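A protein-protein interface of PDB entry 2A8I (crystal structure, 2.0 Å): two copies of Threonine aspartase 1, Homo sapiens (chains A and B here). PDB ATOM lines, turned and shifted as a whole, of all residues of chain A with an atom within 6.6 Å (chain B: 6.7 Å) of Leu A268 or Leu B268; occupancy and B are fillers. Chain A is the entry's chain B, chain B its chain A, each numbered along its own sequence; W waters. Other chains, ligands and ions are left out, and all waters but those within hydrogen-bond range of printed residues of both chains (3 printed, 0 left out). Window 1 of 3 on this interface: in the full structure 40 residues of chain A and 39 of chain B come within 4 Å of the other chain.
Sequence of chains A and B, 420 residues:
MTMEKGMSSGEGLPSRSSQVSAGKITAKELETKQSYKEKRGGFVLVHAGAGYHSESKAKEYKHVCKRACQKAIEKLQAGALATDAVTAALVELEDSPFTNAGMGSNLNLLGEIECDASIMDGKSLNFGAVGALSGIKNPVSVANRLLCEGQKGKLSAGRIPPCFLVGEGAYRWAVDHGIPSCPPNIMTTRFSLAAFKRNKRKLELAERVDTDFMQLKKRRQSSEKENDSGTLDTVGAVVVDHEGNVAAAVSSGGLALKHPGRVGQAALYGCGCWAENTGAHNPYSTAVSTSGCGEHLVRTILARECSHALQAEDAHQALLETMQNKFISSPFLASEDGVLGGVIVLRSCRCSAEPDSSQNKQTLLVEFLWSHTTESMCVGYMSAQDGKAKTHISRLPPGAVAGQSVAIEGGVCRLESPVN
The backbone carbonyl oxygen (O) of Phe B164 is in hydrogen-bond range of the backbone NH (N) of Val A263 (3.1 Å). The backbone carbonyl oxygen (O) of Phe A164 is in hydrogen-bond range of the backbone NH (N) of Val B263 (3.2 Å).
CE2 of Phe A164 touches CD2 of Leu B268, at 3.8 Å. Phe B164 touches Leu A268. Leu A268 touches Leu B268. O of Val B298 touches CE2 of Tyr A269, 3.1 Å away. Val A298 touches Tyr B269 (O to CE2, 3.2 Å).
Of the printed residues of chain B, Phe A164 touches Val B263 (3.2 Å) and Leu B268 (3.8 Å). Leu A268 touches two residues of chain B. Of the printed residues of chain B, Tyr A269 touches Val B298 (3.1 Å). Of the printed residues of chain A, Phe B164 touches Val A263 (3.1 Å) and Leu A268 (3.7 Å). Ala B267 touches none of the printed residues of chain A. Of chain A, only Phe A164 and Leu A268 come within 4 Å of Leu B268. Of the printed residues of chain A, Val B298 touches Tyr A269 (3.1 Å). The nearest residue of chain B that does not touch Leu A268 is Tyr B269 (5.1 Å). The nearest residue of chain A that does not touch Leu B268 is Tyr A269 (5.0 Å). The nearest printed residue of chain B that does not touch Tyr A269 is Cys B271 (4.9 Å).
Hydrophobic or aromatic side chains of chain A within 4 Å of the printed part of chain B: Phe A164, Val A263, Leu A268 and Tyr A269. Among the printed residues, 7 pairs touch across the chains. Among the printed residues, no Asp or Glu carboxylate lies within 4 Å of a Lys or Arg side-chain nitrogen of the other chain.
Phe A164 touches Val B263, and with the chains exchanged Val A263 touches Phe B164. Phe A164 touches Leu B268, and with the chains exchanged Leu A268 touches Phe B164. Leu A268 touches its own counterpart, Leu B268. Tyr A269 touches Val B298, and with the chains exchanged Val A298 touches Tyr B269. 20 positions are printed for both chains. Of the 7 pairs that touch across the chains among the printed residues, 7 have their exchanged pair printed and touching as well.
Water W2 lies within hydrogen-bond range of O of Tyr A269 (2.9 Å) and O of Tyr B269 (3.2 Å). Water W3 lies within hydrogen-bond range of the backbone NH (N) of Phe B164, the backbone NH (N) of Cys B163 and the backbone carbonyl oxygen (O) of Val A263. Water W1 lies within hydrogen-bond range of N of Phe A164 (3.2 Å), O of Val B263 (3.3 Å) and N of Cys A163 (3.3 Å).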
ATOM      1  N   ASP A 116      -9.622   1.144 -10.547  1.00  0.00           N
ATOM      2  CA  ASP A 116     -10.580   0.048 -10.396  1.00  0.00           C
ATOM      3  C   ASP A 116      -9.873  -0.995  -9.529  1.00  0.00           C
ATOM      4  O   ASP A 116      -8.667  -1.217  -9.669  1.00  0.00           O
ATOM      5  CB  ASP A 116     -10.945  -0.603 -11.746  1.00  0.00           C
ATOM      6  CG  ASP A 116     -11.582   0.370 -12.738  1.00  0.00           C
ATOM      7  OD1 ASP A 116     -12.232   1.345 -12.311  1.00  0.00           O
ATOM      8  OD2 ASP A 116     -11.448   0.140 -13.964  1.00  0.00           O
ATOM      9  N   ALA A 117     -10.616  -1.632  -8.635  1.00  0.00           N
ATOM     10  CA  ALA A 117     -10.048  -2.654  -7.765  1.00  0.00           C
ATOM     11  C   ALA A 117     -11.154  -3.494  -7.164  1.00  0.00           C
ATOM     12  O   ALA A 117     -12.264  -3.005  -6.936  1.00  0.00           O
ATOM     13  CB  ALA A 117      -9.228  -2.009  -6.646  1.00  0.00           C
ATOM     14  N   SER A 118     -10.858  -4.761  -6.915  1.00  0.00           N
ATOM     15  CA  SER A 118     -11.843  -5.636  -6.314  1.00  0.00           C
ATOM     16  C   SER A 118     -11.149  -6.740  -5.532  1.00  0.00           C
ATOM     17  O   SER A 118      -9.955  -7.000  -5.712  1.00  0.00           O
ATOM     18  CB  SER A 118     -12.764  -6.234  -7.395  1.00  0.00           C
ATOM     19  OG  SER A 118     -12.047  -7.079  -8.280  1.00  0.00           O
ATOM     20  N   PHE A 127     -17.775 -10.232  -1.590  1.00  0.00           N
ATOM     21  CA  PHE A 127     -17.033  -9.457  -2.571  1.00  0.00           C
ATOM     22  C   PHE A 127     -17.013  -7.970  -2.228  1.00  0.00           C
ATOM     23  O   PHE A 127     -17.918  -7.474  -1.564  1.00  0.00           O
ATOM     24  CB  PHE A 127     -17.746  -9.697  -3.910  1.00  0.00           C
ATOM     25  CG  PHE A 127     -17.194  -8.940  -5.076  1.00  0.00           C
ATOM     26  CD1 PHE A 127     -16.023  -9.352  -5.701  1.00  0.00           C
ATOM     27  CD2 PHE A 127     -17.905  -7.875  -5.623  1.00  0.00           C
ATOM     28  CE1 PHE A 127     -15.569  -8.721  -6.861  1.00  0.00           C
ATOM     29  CE2 PHE A 127     -17.460  -7.238  -6.783  1.00  0.00           C
ATOM     30  CZ  PHE A 127     -16.287  -7.666  -7.405  1.00  0.00           C
ATOM     31  N   ALA A 129     -15.715  -4.091  -4.178  1.00  0.00           N
ATOM     32  CA  ALA A 129     -15.144  -3.472  -5.371  1.00  0.00           C
ATOM     33  C   ALA A 129     -15.361  -1.970  -5.496  1.00  0.00           C
ATOM     34  O   ALA A 129     -16.326  -1.424  -4.971  1.00  0.00           O
ATOM     35  CB  ALA A 129     -15.696  -4.163  -6.613  1.00  0.00           C
ATOM     36  N   VAL A 130     -14.450  -1.308  -6.201  1.00  0.00           N
ATOM     37  CA  VAL A 130     -14.564   0.127  -6.442  1.00  0.00           C
ATOM     38  C   VAL A 130     -14.177   0.410  -7.886  1.00  0.00           C
ATOM     39  O   VAL A 130     -13.263  -0.221  -8.425  1.00  0.00           O
ATOM     40  CB  VAL A 130     -13.651   0.980  -5.509  1.00  0.00           C
ATOM     41  CG1 VAL A 130     -14.064   0.805  -4.068  1.00  0.00           C
ATOM     42  CG2 VAL A 130     -12.194   0.606  -5.695  1.00  0.00           C
ATOM     43  N   CYS A 163     -21.493  -3.683  -2.149  1.00  0.00           N
ATOM     44  CA  CYS A 163     -20.264  -4.407  -2.444  1.00  0.00           C
ATOM     45  C   CYS A 163     -19.546  -3.700  -3.585  1.00  0.00           C
ATOM     46  O   CYS A 163     -18.389  -3.997  -3.871  1.00  0.00           O
ATOM     47  CB  CYS A 163     -20.558  -5.859  -2.843  1.00  0.00           C
ATOM     48  SG  CYS A 163     -21.543  -6.054  -4.351  1.00  0.00           S
ATOM     49  N   PHE A 164     -20.224  -2.739  -4.212  1.00  0.00           N
ATOM     50  CA  PHE A 164     -19.655  -2.013  -5.342  1.00  0.00           C
ATOM     51  C   PHE A 164     -19.998  -0.520  -5.365  1.00  0.00           C
ATOM     52  O   PHE A 164     -21.155  -0.147  -5.542  1.00  0.00           O
ATOM     53  CB  PHE A 164     -20.130  -2.679  -6.640  1.00  0.00           C
ATOM     54  CG  PHE A 164     -19.535  -2.103  -7.889  1.00  0.00           C
ATOM     55  CD1 PHE A 164     -18.252  -1.558  -7.889  1.00  0.00           C
ATOM     56  CD2 PHE A 164     -20.230  -2.174  -9.093  1.00  0.00           C
ATOM     57  CE1 PHE A 164     -17.667  -1.097  -9.065  1.00  0.00           C
ATOM     58  CE2 PHE A 164     -19.655  -1.716 -10.282  1.00  0.00           C
ATOM     59  CZ  PHE A 164     -18.368  -1.177 -10.268  1.00  0.00           C
ATOM     60  N   VAL A 263     -15.073   2.294 -16.567  1.00  0.00           N
ATOM     61  CA  VAL A 263     -14.743   1.270 -15.583  1.00  0.00           C
ATOM     62  C   VAL A 263     -14.330   0.008 -16.320  1.00  0.00           C
ATOM     63  O   VAL A 263     -14.935  -0.347 -17.320  1.00  0.00           O
ATOM     64  CB  VAL A 263     -15.952   0.990 -14.667  1.00  0.00           C
ATOM     65  CG1 VAL A 263     -15.667  -0.178 -13.750  1.00  0.00           C
ATOM     66  CG2 VAL A 263     -16.257   2.234 -13.841  1.00  0.00           C
ATOM     67  N   GLY A 264     -13.297  -0.659 -15.818  1.00  0.00           N
ATOM     68  CA  GLY A 264     -12.801  -1.859 -16.463  1.00  0.00           C
ATOM     69  C   GLY A 264     -12.959  -3.165 -15.705  1.00  0.00           C
ATOM     70  O   GLY A 264     -13.695  -3.259 -14.725  1.00  0.00           O
ATOM     71  N   GLN A 265     -12.219  -4.172 -16.157  1.00  0.00           N
ATOM     72  CA  GLN A 265     -12.282  -5.511 -15.598  1.00  0.00           C
ATOM     73  C   GLN A 265     -11.994  -5.645 -14.110  1.00  0.00           C
ATOM     74  O   GLN A 265     -12.643  -6.424 -13.418  1.00  0.00           O
ATOM     75  CB  GLN A 265     -11.354  -6.427 -16.410  1.00  0.00           C
ATOM     76  CG  GLN A 265      -9.872  -6.031 -16.369  1.00  0.00           C
ATOM     77  CD  GLN A 265      -9.139  -6.823 -15.335  1.00  0.00           C
ATOM     78  OE1 GLN A 265      -7.984  -6.543 -15.010  1.00  0.00           O
ATOM     79  NE2 GLN A 265      -9.810  -7.842 -14.806  1.00  0.00           N
ATOM     80  N   ALA A 266     -11.032  -4.883 -13.612  1.00  0.00           N
ATOM     81  CA  ALA A 266     -10.661  -4.944 -12.209  1.00  0.00           C
ATOM     82  C   ALA A 266     -11.776  -4.627 -11.211  1.00  0.00           C
ATOM     83  O   ALA A 266     -11.662  -4.964 -10.037  1.00  0.00           O
ATOM     84  CB  ALA A 266      -9.477  -4.033 -11.958  1.00  0.00           C
ATOM     85  N   ALA A 267     -12.851  -3.993 -11.669  1.00  0.00           N
ATOM     86  CA  ALA A 267     -13.953  -3.642 -10.776  1.00  0.00           C
ATOM     87  C   ALA A 267     -15.180  -4.541 -10.896  1.00  0.00           C
ATOM     88  O   ALA A 267     -16.035  -4.563 -10.003  1.00  0.00           O
ATOM     89  CB  ALA A 267     -14.368  -2.202 -11.022  1.00  0.00           C
ATOM     90  N   LEU A 268     -15.262  -5.291 -11.985  1.00  0.00           N
ATOM     91  CA  LEU A 268     -16.428  -6.131 -12.239  1.00  0.00           C
ATOM     92  C   LEU A 268     -16.411  -7.555 -11.708  1.00  0.00           C
ATOM     93  O   LEU A 268     -15.480  -8.327 -11.973  1.00  0.00           O
ATOM     94  CB  LEU A 268     -16.701  -6.171 -13.741  1.00  0.00           C
ATOM     95  CG  LEU A 268     -16.778  -4.809 -14.419  1.00  0.00           C
ATOM     96  CD1 LEU A 268     -16.921  -5.002 -15.928  1.00  0.00           C
ATOM     97  CD2 LEU A 268     -17.954  -4.020 -13.845  1.00  0.00           C
ATOM     98  N   TYR A 269     -17.475  -7.888 -10.982  1.00  0.00           N
ATOM     99  CA  TYR A 269     -17.684  -9.213 -10.396  1.00  0.00           C
ATOM    100  C   TYR A 269     -17.561 -10.307 -11.467  1.00  0.00           C
ATOM    101  O   TYR A 269     -18.225 -10.256 -12.505  1.00  0.00           O
ATOM    102  CB  TYR A 269     -19.082  -9.266  -9.773  1.00  0.00           C
ATOM    103  CG  TYR A 269     -19.391 -10.507  -8.971  1.00  0.00           C
ATOM    104  CD1 TYR A 269     -18.734 -10.766  -7.769  1.00  0.00           C
ATOM    105  CD2 TYR A 269     -20.385 -11.397  -9.386  1.00  0.00           C
ATOM    106  CE1 TYR A 269     -19.068 -11.874  -6.993  1.00  0.00           C
ATOM    107  CE2 TYR A 269     -20.727 -12.507  -8.622  1.00  0.00           C
ATOM    108  CZ  TYR A 269     -20.070 -12.737  -7.426  1.00  0.00           C
ATOM    109  OH  TYR A 269     -20.440 -13.806  -6.649  1.00  0.00           O
ATOM    110  N   GLY A 270     -16.709 -11.293 -11.208  1.00  0.00           N
ATOM    111  CA  GLY A 270     -16.523 -12.384 -12.152  1.00  0.00           C
ATOM    112  C   GLY A 270     -15.444 -12.165 -13.194  1.00  0.00           C
ATOM    113  O   GLY A 270     -14.894 -13.125 -13.742  1.00  0.00           O
ATOM    114  N   CYS A 271     -15.119 -10.906 -13.460  1.00  0.00           N
ATOM    115  CA  CYS A 271     -14.124 -10.576 -14.469  1.00  0.00           C
ATOM    116  C   CYS A 271     -12.706 -10.330 -13.948  1.00  0.00           C
ATOM    117  O   CYS A 271     -11.747 -10.903 -14.472  1.00  0.00           O
ATOM    118  CB  CYS A 271     -14.608  -9.366 -15.266  1.00  0.00           C
ATOM    119  SG  CYS A 271     -16.299  -9.579 -15.898  1.00  0.00           S
ATOM    120  N   GLY A 272     -12.573  -9.500 -12.916  1.00  0.00           N
ATOM    121  CA  GLY A 272     -11.258  -9.186 -12.377  1.00  0.00           C
ATOM    122  C   GLY A 272     -10.574 -10.260 -11.545  1.00  0.00           C
ATOM    123  O   GLY A 272      -9.403 -10.585 -11.774  1.00  0.00           O
ATOM    124  N   CYS A 273     -11.295 -10.790 -10.564  1.00  0.00           N
ATOM    125  CA  CYS A 273     -10.772 -11.824  -9.698  1.00  0.00           C
ATOM    126  C   CYS A 273     -11.905 -12.744  -9.289  1.00  0.00           C
ATOM    127  O   CYS A 273     -13.071 -12.464  -9.558  1.00  0.00           O
ATOM    128  CB  CYS A 273     -10.129 -11.211  -8.448  1.00  0.00           C
ATOM    129  SG  CYS A 273     -11.279 -10.342  -7.351  1.00  0.00           S
ATOM    130  N   VAL A 298     -13.309  -8.756 -19.693  1.00  0.00           N
ATOM    131  CA  VAL A 298     -14.701  -8.543 -19.333  1.00  0.00           C
ATOM    132  C   VAL A 298     -15.664  -9.338 -20.214  1.00  0.00           C
ATOM    133  O   VAL A 298     -16.523 -10.057 -19.701  1.00  0.00           O
ATOM    134  CB  VAL A 298     -15.080  -7.043 -19.416  1.00  0.00           C
ATOM    135  CG1 VAL A 298     -16.586  -6.875 -19.271  1.00  0.00           C
ATOM    136  CG2 VAL A 298     -14.363  -6.266 -18.317  1.00  0.00           C
ATOM    137  N   ASP B 116     -28.968   2.946 -13.152  1.00  0.00           N
ATOM    138  CA  ASP B 116     -28.154   1.887 -13.732  1.00  0.00           C
ATOM    139  C   ASP B 116     -28.949   1.309 -14.899  1.00  0.00           C
ATOM    140  O   ASP B 116     -30.160   1.075 -14.779  1.00  0.00           O
ATOM    141  CB  ASP B 116     -27.899   0.760 -12.726  1.00  0.00           C
ATOM    142  CG  ASP B 116     -27.231   1.236 -11.452  1.00  0.00           C
ATOM    143  OD1 ASP B 116     -26.415   2.176 -11.520  1.00  0.00           O
ATOM    144  OD2 ASP B 116     -27.513   0.649 -10.383  1.00  0.00           O
ATOM    145  N   ALA B 117     -28.280   1.072 -16.020  1.00  0.00           N
ATOM    146  CA  ALA B 117     -28.944   0.500 -17.188  1.00  0.00           C
ATOM    147  C   ALA B 117     -27.930  -0.209 -18.074  1.00  0.00           C
ATOM    148  O   ALA B 117     -26.758   0.157 -18.091  1.00  0.00           O
ATOM    149  CB  ALA B 117     -29.668   1.599 -17.981  1.00  0.00           C
ATOM    150  N   SER B 118     -28.381  -1.227 -18.801  1.00  0.00           N
ATOM    151  CA  SER B 118     -27.506  -1.969 -19.706  1.00  0.00           C
ATOM    152  C   SER B 118     -28.314  -2.610 -20.827  1.00  0.00           C
ATOM    153  O   SER B 118     -29.533  -2.739 -20.730  1.00  0.00           O
ATOM    154  CB  SER B 118     -26.703  -3.039 -18.942  1.00  0.00           C
ATOM    155  OG  SER B 118     -27.525  -4.049 -18.380  1.00  0.00           O
ATOM    156  N   PHE B 127     -22.053  -5.042 -25.971  1.00  0.00           N
ATOM    157  CA  PHE B 127     -22.722  -4.613 -24.753  1.00  0.00           C
ATOM    158  C   PHE B 127     -22.553  -3.115 -24.487  1.00  0.00           C
ATOM    159  O   PHE B 127     -21.597  -2.502 -24.952  1.00  0.00           O
ATOM    160  CB  PHE B 127     -22.098  -5.440 -23.622  1.00  0.00           C
ATOM    161  CG  PHE B 127     -22.550  -5.073 -22.246  1.00  0.00           C
ATOM    162  CD1 PHE B 127     -23.790  -5.479 -21.777  1.00  0.00           C
ATOM    163  CD2 PHE B 127     -21.694  -4.384 -21.385  1.00  0.00           C
ATOM    164  CE1 PHE B 127     -24.178  -5.213 -20.465  1.00  0.00           C
ATOM    165  CE2 PHE B 127     -22.066  -4.112 -20.078  1.00  0.00           C
ATOM    166  CZ  PHE B 127     -23.312  -4.529 -19.611  1.00  0.00           C
ATOM    167  N   ALA B 129     -23.487  -0.126 -21.134  1.00  0.00           N
ATOM    168  CA  ALA B 129     -24.053   0.078 -19.805  1.00  0.00           C
ATOM    169  C   ALA B 129     -23.562   1.322 -19.072  1.00  0.00           C
ATOM    170  O   ALA B 129     -22.453   1.808 -19.297  1.00  0.00           O
ATOM    171  CB  ALA B 129     -23.785  -1.147 -18.944  1.00  0.00           C
ATOM    172  N   VAL B 130     -24.407   1.818 -18.178  1.00  0.00           N
ATOM    173  CA  VAL B 130     -24.082   2.976 -17.376  1.00  0.00           C
ATOM    174  C   VAL B 130     -24.458   2.692 -15.929  1.00  0.00           C
ATOM    175  O   VAL B 130     -25.409   1.956 -15.659  1.00  0.00           O
ATOM    176  CB  VAL B 130     -24.824   4.253 -17.877  1.00  0.00           C
ATOM    177  CG1 VAL B 130     -24.324   4.628 -19.257  1.00  0.00           C
ATOM    178  CG2 VAL B 130     -26.331   4.027 -17.899  1.00  0.00           C
ATOM    179  N   CYS B 163     -17.472   0.342 -22.941  1.00  0.00           N
ATOM    180  CA  CYS B 163     -18.760  -0.328 -22.933  1.00  0.00           C
ATOM    181  C   CYS B 163     -19.468   0.010 -21.621  1.00  0.00           C
ATOM    182  O   CYS B 163     -20.685  -0.118 -21.512  1.00  0.00           O
ATOM    183  CB  CYS B 163     -18.600  -1.849 -23.081  1.00  0.00           C
ATOM    184  SG  CYS B 163     -17.772  -2.728 -21.725  1.00  0.00           S
ATOM    185  N   PHE B 164     -18.700   0.484 -20.643  1.00  0.00           N
ATOM    186  CA  PHE B 164     -19.243   0.807 -19.327  1.00  0.00           C
ATOM    187  C   PHE B 164     -18.701   2.118 -18.754  1.00  0.00           C
ATOM    188  O   PHE B 164     -17.502   2.256 -18.519  1.00  0.00           O
ATOM    189  CB  PHE B 164     -18.948  -0.370 -18.381  1.00  0.00           C
ATOM    190  CG  PHE B 164     -19.504  -0.216 -16.987  1.00  0.00           C
ATOM    191  CD1 PHE B 164     -20.711   0.440 -16.759  1.00  0.00           C
ATOM    192  CD2 PHE B 164     -18.848  -0.801 -15.906  1.00  0.00           C
ATOM    193  CE1 PHE B 164     -21.256   0.506 -15.479  1.00  0.00           C
ATOM    194  CE2 PHE B 164     -19.389  -0.740 -14.618  1.00  0.00           C
ATOM    195  CZ  PHE B 164     -20.591  -0.088 -14.406  1.00  0.00           C
ATOM    196  N   VAL B 263     -23.645   0.865  -7.323  1.00  0.00           N
ATOM    197  CA  VAL B 263     -24.061   0.345  -8.613  1.00  0.00           C
ATOM    198  C   VAL B 263     -24.661  -1.036  -8.430  1.00  0.00           C
ATOM    199  O   VAL B 263     -24.092  -1.877  -7.740  1.00  0.00           O
ATOM    200  CB  VAL B 263     -22.874   0.279  -9.571  1.00  0.00           C
ATOM    201  CG1 VAL B 263     -23.284  -0.378 -10.885  1.00  0.00           C
ATOM    202  CG2 VAL B 263     -22.360   1.689  -9.818  1.00  0.00           C
ATOM    203  N   GLY B 264     -25.820  -1.252  -9.047  1.00  0.00           N
ATOM    204  CA  GLY B 264     -26.506  -2.526  -8.928  1.00  0.00           C
ATOM    205  C   GLY B 264     -26.419  -3.428 -10.142  1.00  0.00           C
ATOM    206  O   GLY B 264     -25.676  -3.158 -11.089  1.00  0.00           O
ATOM    207  N   GLN B 265     -27.201  -4.501 -10.114  1.00  0.00           N
ATOM    208  CA  GLN B 265     -27.200  -5.487 -11.186  1.00  0.00           C
ATOM    209  C   GLN B 265     -27.538  -4.969 -12.582  1.00  0.00           C
ATOM    210  O   GLN B 265     -27.059  -5.514 -13.572  1.00  0.00           O
ATOM    211  CB  GLN B 265     -28.141  -6.651 -10.827  1.00  0.00           C
ATOM    212  CG  GLN B 265     -29.388  -6.785 -11.703  1.00  0.00           C
ATOM    213  CD  GLN B 265     -30.477  -5.799 -11.333  1.00  0.00           C
ATOM    214  OE1 GLN B 265     -30.266  -4.902 -10.516  1.00  0.00           O
ATOM    215  NE2 GLN B 265     -31.654  -5.958 -11.939  1.00  0.00           N
ATOM    216  N   ALA B 266     -28.346  -3.918 -12.671  1.00  0.00           N
ATOM    217  CA  ALA B 266     -28.736  -3.401 -13.978  1.00  0.00           C
ATOM    218  C   ALA B 266     -27.573  -2.862 -14.820  1.00  0.00           C
ATOM    219  O   ALA B 266     -27.702  -2.699 -16.034  1.00  0.00           O
ATOM    220  CB  ALA B 266     -29.823  -2.334 -13.819  1.00  0.00           C
ATOM    221  N   ALA B 267     -26.431  -2.607 -14.191  1.00  0.00           N
ATOM    222  CA  ALA B 267     -25.279  -2.099 -14.921  1.00  0.00           C
ATOM    223  C   ALA B 267     -24.191  -3.149 -15.138  1.00  0.00           C
ATOM    224  O   ALA B 267     -23.290  -2.950 -15.937  1.00  0.00           O
ATOM    225  CB  ALA B 267     -24.686  -0.891 -14.182  1.00  0.00           C
ATOM    226  N   LEU B 268     -24.289  -4.276 -14.442  1.00  0.00           N
ATOM    227  CA  LEU B 268     -23.258  -5.305 -14.519  1.00  0.00           C
ATOM    228  C   LEU B 268     -23.391  -6.377 -15.593  1.00  0.00           C
ATOM    229  O   LEU B 268     -24.395  -7.097 -15.663  1.00  0.00           O
ATOM    230  CB  LEU B 268     -23.114  -5.971 -13.151  1.00  0.00           C
ATOM    231  CG  LEU B 268     -22.637  -5.028 -12.046  1.00  0.00           C
ATOM    232  CD1 LEU B 268     -22.533  -5.779 -10.727  1.00  0.00           C
ATOM    233  CD2 LEU B 268     -21.288  -4.446 -12.437  1.00  0.00           C
ATOM    234  N   TYR B 269     -22.348  -6.475 -16.416  1.00  0.00           N
ATOM    235  CA  TYR B 269     -22.279  -7.446 -17.501  1.00  0.00           C
ATOM    236  C   TYR B 269     -22.594  -8.838 -16.959  1.00  0.00           C
ATOM    237  O   TYR B 269     -22.024  -9.268 -15.958  1.00  0.00           O
ATOM    238  CB  TYR B 269     -20.872  -7.426 -18.111  1.00  0.00           C
ATOM    239  CG  TYR B 269     -20.680  -8.303 -19.327  1.00  0.00           C
ATOM    240  CD1 TYR B 269     -21.250  -7.964 -20.554  1.00  0.00           C
ATOM    241  CD2 TYR B 269     -19.893  -9.455 -19.259  1.00  0.00           C
ATOM    242  CE1 TYR B 269     -21.037  -8.745 -21.688  1.00  0.00           C
ATOM    243  CE2 TYR B 269     -19.673 -10.247 -20.386  1.00  0.00           C
ATOM    244  CZ  TYR B 269     -20.248  -9.884 -21.599  1.00  0.00           C
ATOM    245  OH  TYR B 269     -20.024 -10.652 -22.717  1.00  0.00           O
ATOM    246  N   GLY B 270     -23.523  -9.523 -17.618  1.00  0.00           N
ATOM    247  CA  GLY B 270     -23.902 -10.863 -17.210  1.00  0.00           C
ATOM    248  C   GLY B 270     -24.909 -10.973 -16.077  1.00  0.00           C
ATOM    249  O   GLY B 270     -25.531 -12.024 -15.900  1.00  0.00           O
ATOM    250  N   CYS B 271     -25.090  -9.898 -15.319  1.00  0.00           N
ATOM    251  CA  CYS B 271     -26.007  -9.926 -14.187  1.00  0.00           C
ATOM    252  C   CYS B 271     -27.388  -9.386 -14.493  1.00  0.00           C
ATOM    253  O   CYS B 271     -28.386 -10.036 -14.204  1.00  0.00           O
ATOM    254  CB  CYS B 271     -25.415  -9.142 -13.010  1.00  0.00           C
ATOM    255  SG  CYS B 271     -23.751  -9.676 -12.535  1.00  0.00           S
ATOM    256  N   GLY B 272     -27.444  -8.193 -15.078  1.00  0.00           N
ATOM    257  CA  GLY B 272     -28.721  -7.572 -15.381  1.00  0.00           C
ATOM    258  C   GLY B 272     -29.467  -8.116 -16.582  1.00  0.00           C
ATOM    259  O   GLY B 272     -30.673  -8.349 -16.511  1.00  0.00           O
ATOM    260  N   CYS B 273     -28.761  -8.307 -17.691  1.00  0.00           N
ATOM    261  CA  CYS B 273     -29.389  -8.821 -18.895  1.00  0.00           C
ATOM    262  C   CYS B 273     -28.374  -9.625 -19.674  1.00  0.00           C
ATOM    263  O   CYS B 273     -27.192  -9.638 -19.336  1.00  0.00           O
ATOM    264  CB  CYS B 273     -29.918  -7.667 -19.760  1.00  0.00           C
ATOM    265  SG  CYS B 273     -28.656  -6.610 -20.525  1.00  0.00           S
ATOM    266  N   VAL B 298     -26.667 -10.185  -8.670  1.00  0.00           N
ATOM    267  CA  VAL B 298     -25.250 -10.015  -8.944  1.00  0.00           C
ATOM    268  C   VAL B 298     -24.438 -11.217  -8.478  1.00  0.00           C
ATOM    269  O   VAL B 298     -23.725 -11.823  -9.271  1.00  0.00           O
ATOM    270  CB  VAL B 298     -24.674  -8.737  -8.267  1.00  0.00           C
ATOM    271  CG1 VAL B 298     -23.168  -8.638  -8.534  1.00  0.00           C
ATOM    272  CG2 VAL B 298     -25.376  -7.493  -8.797  1.00  0.00           C
HETATM  273  O   HOH W   1     -23.370  -2.630  -4.660  1.00  0.00           O
HETATM  274  O   HOH W   2     -19.694  -8.201 -13.996  1.00  0.00           O
HETATM  275  O   HOH W   3     -15.620   0.268 -20.454  1.00  0.00           O
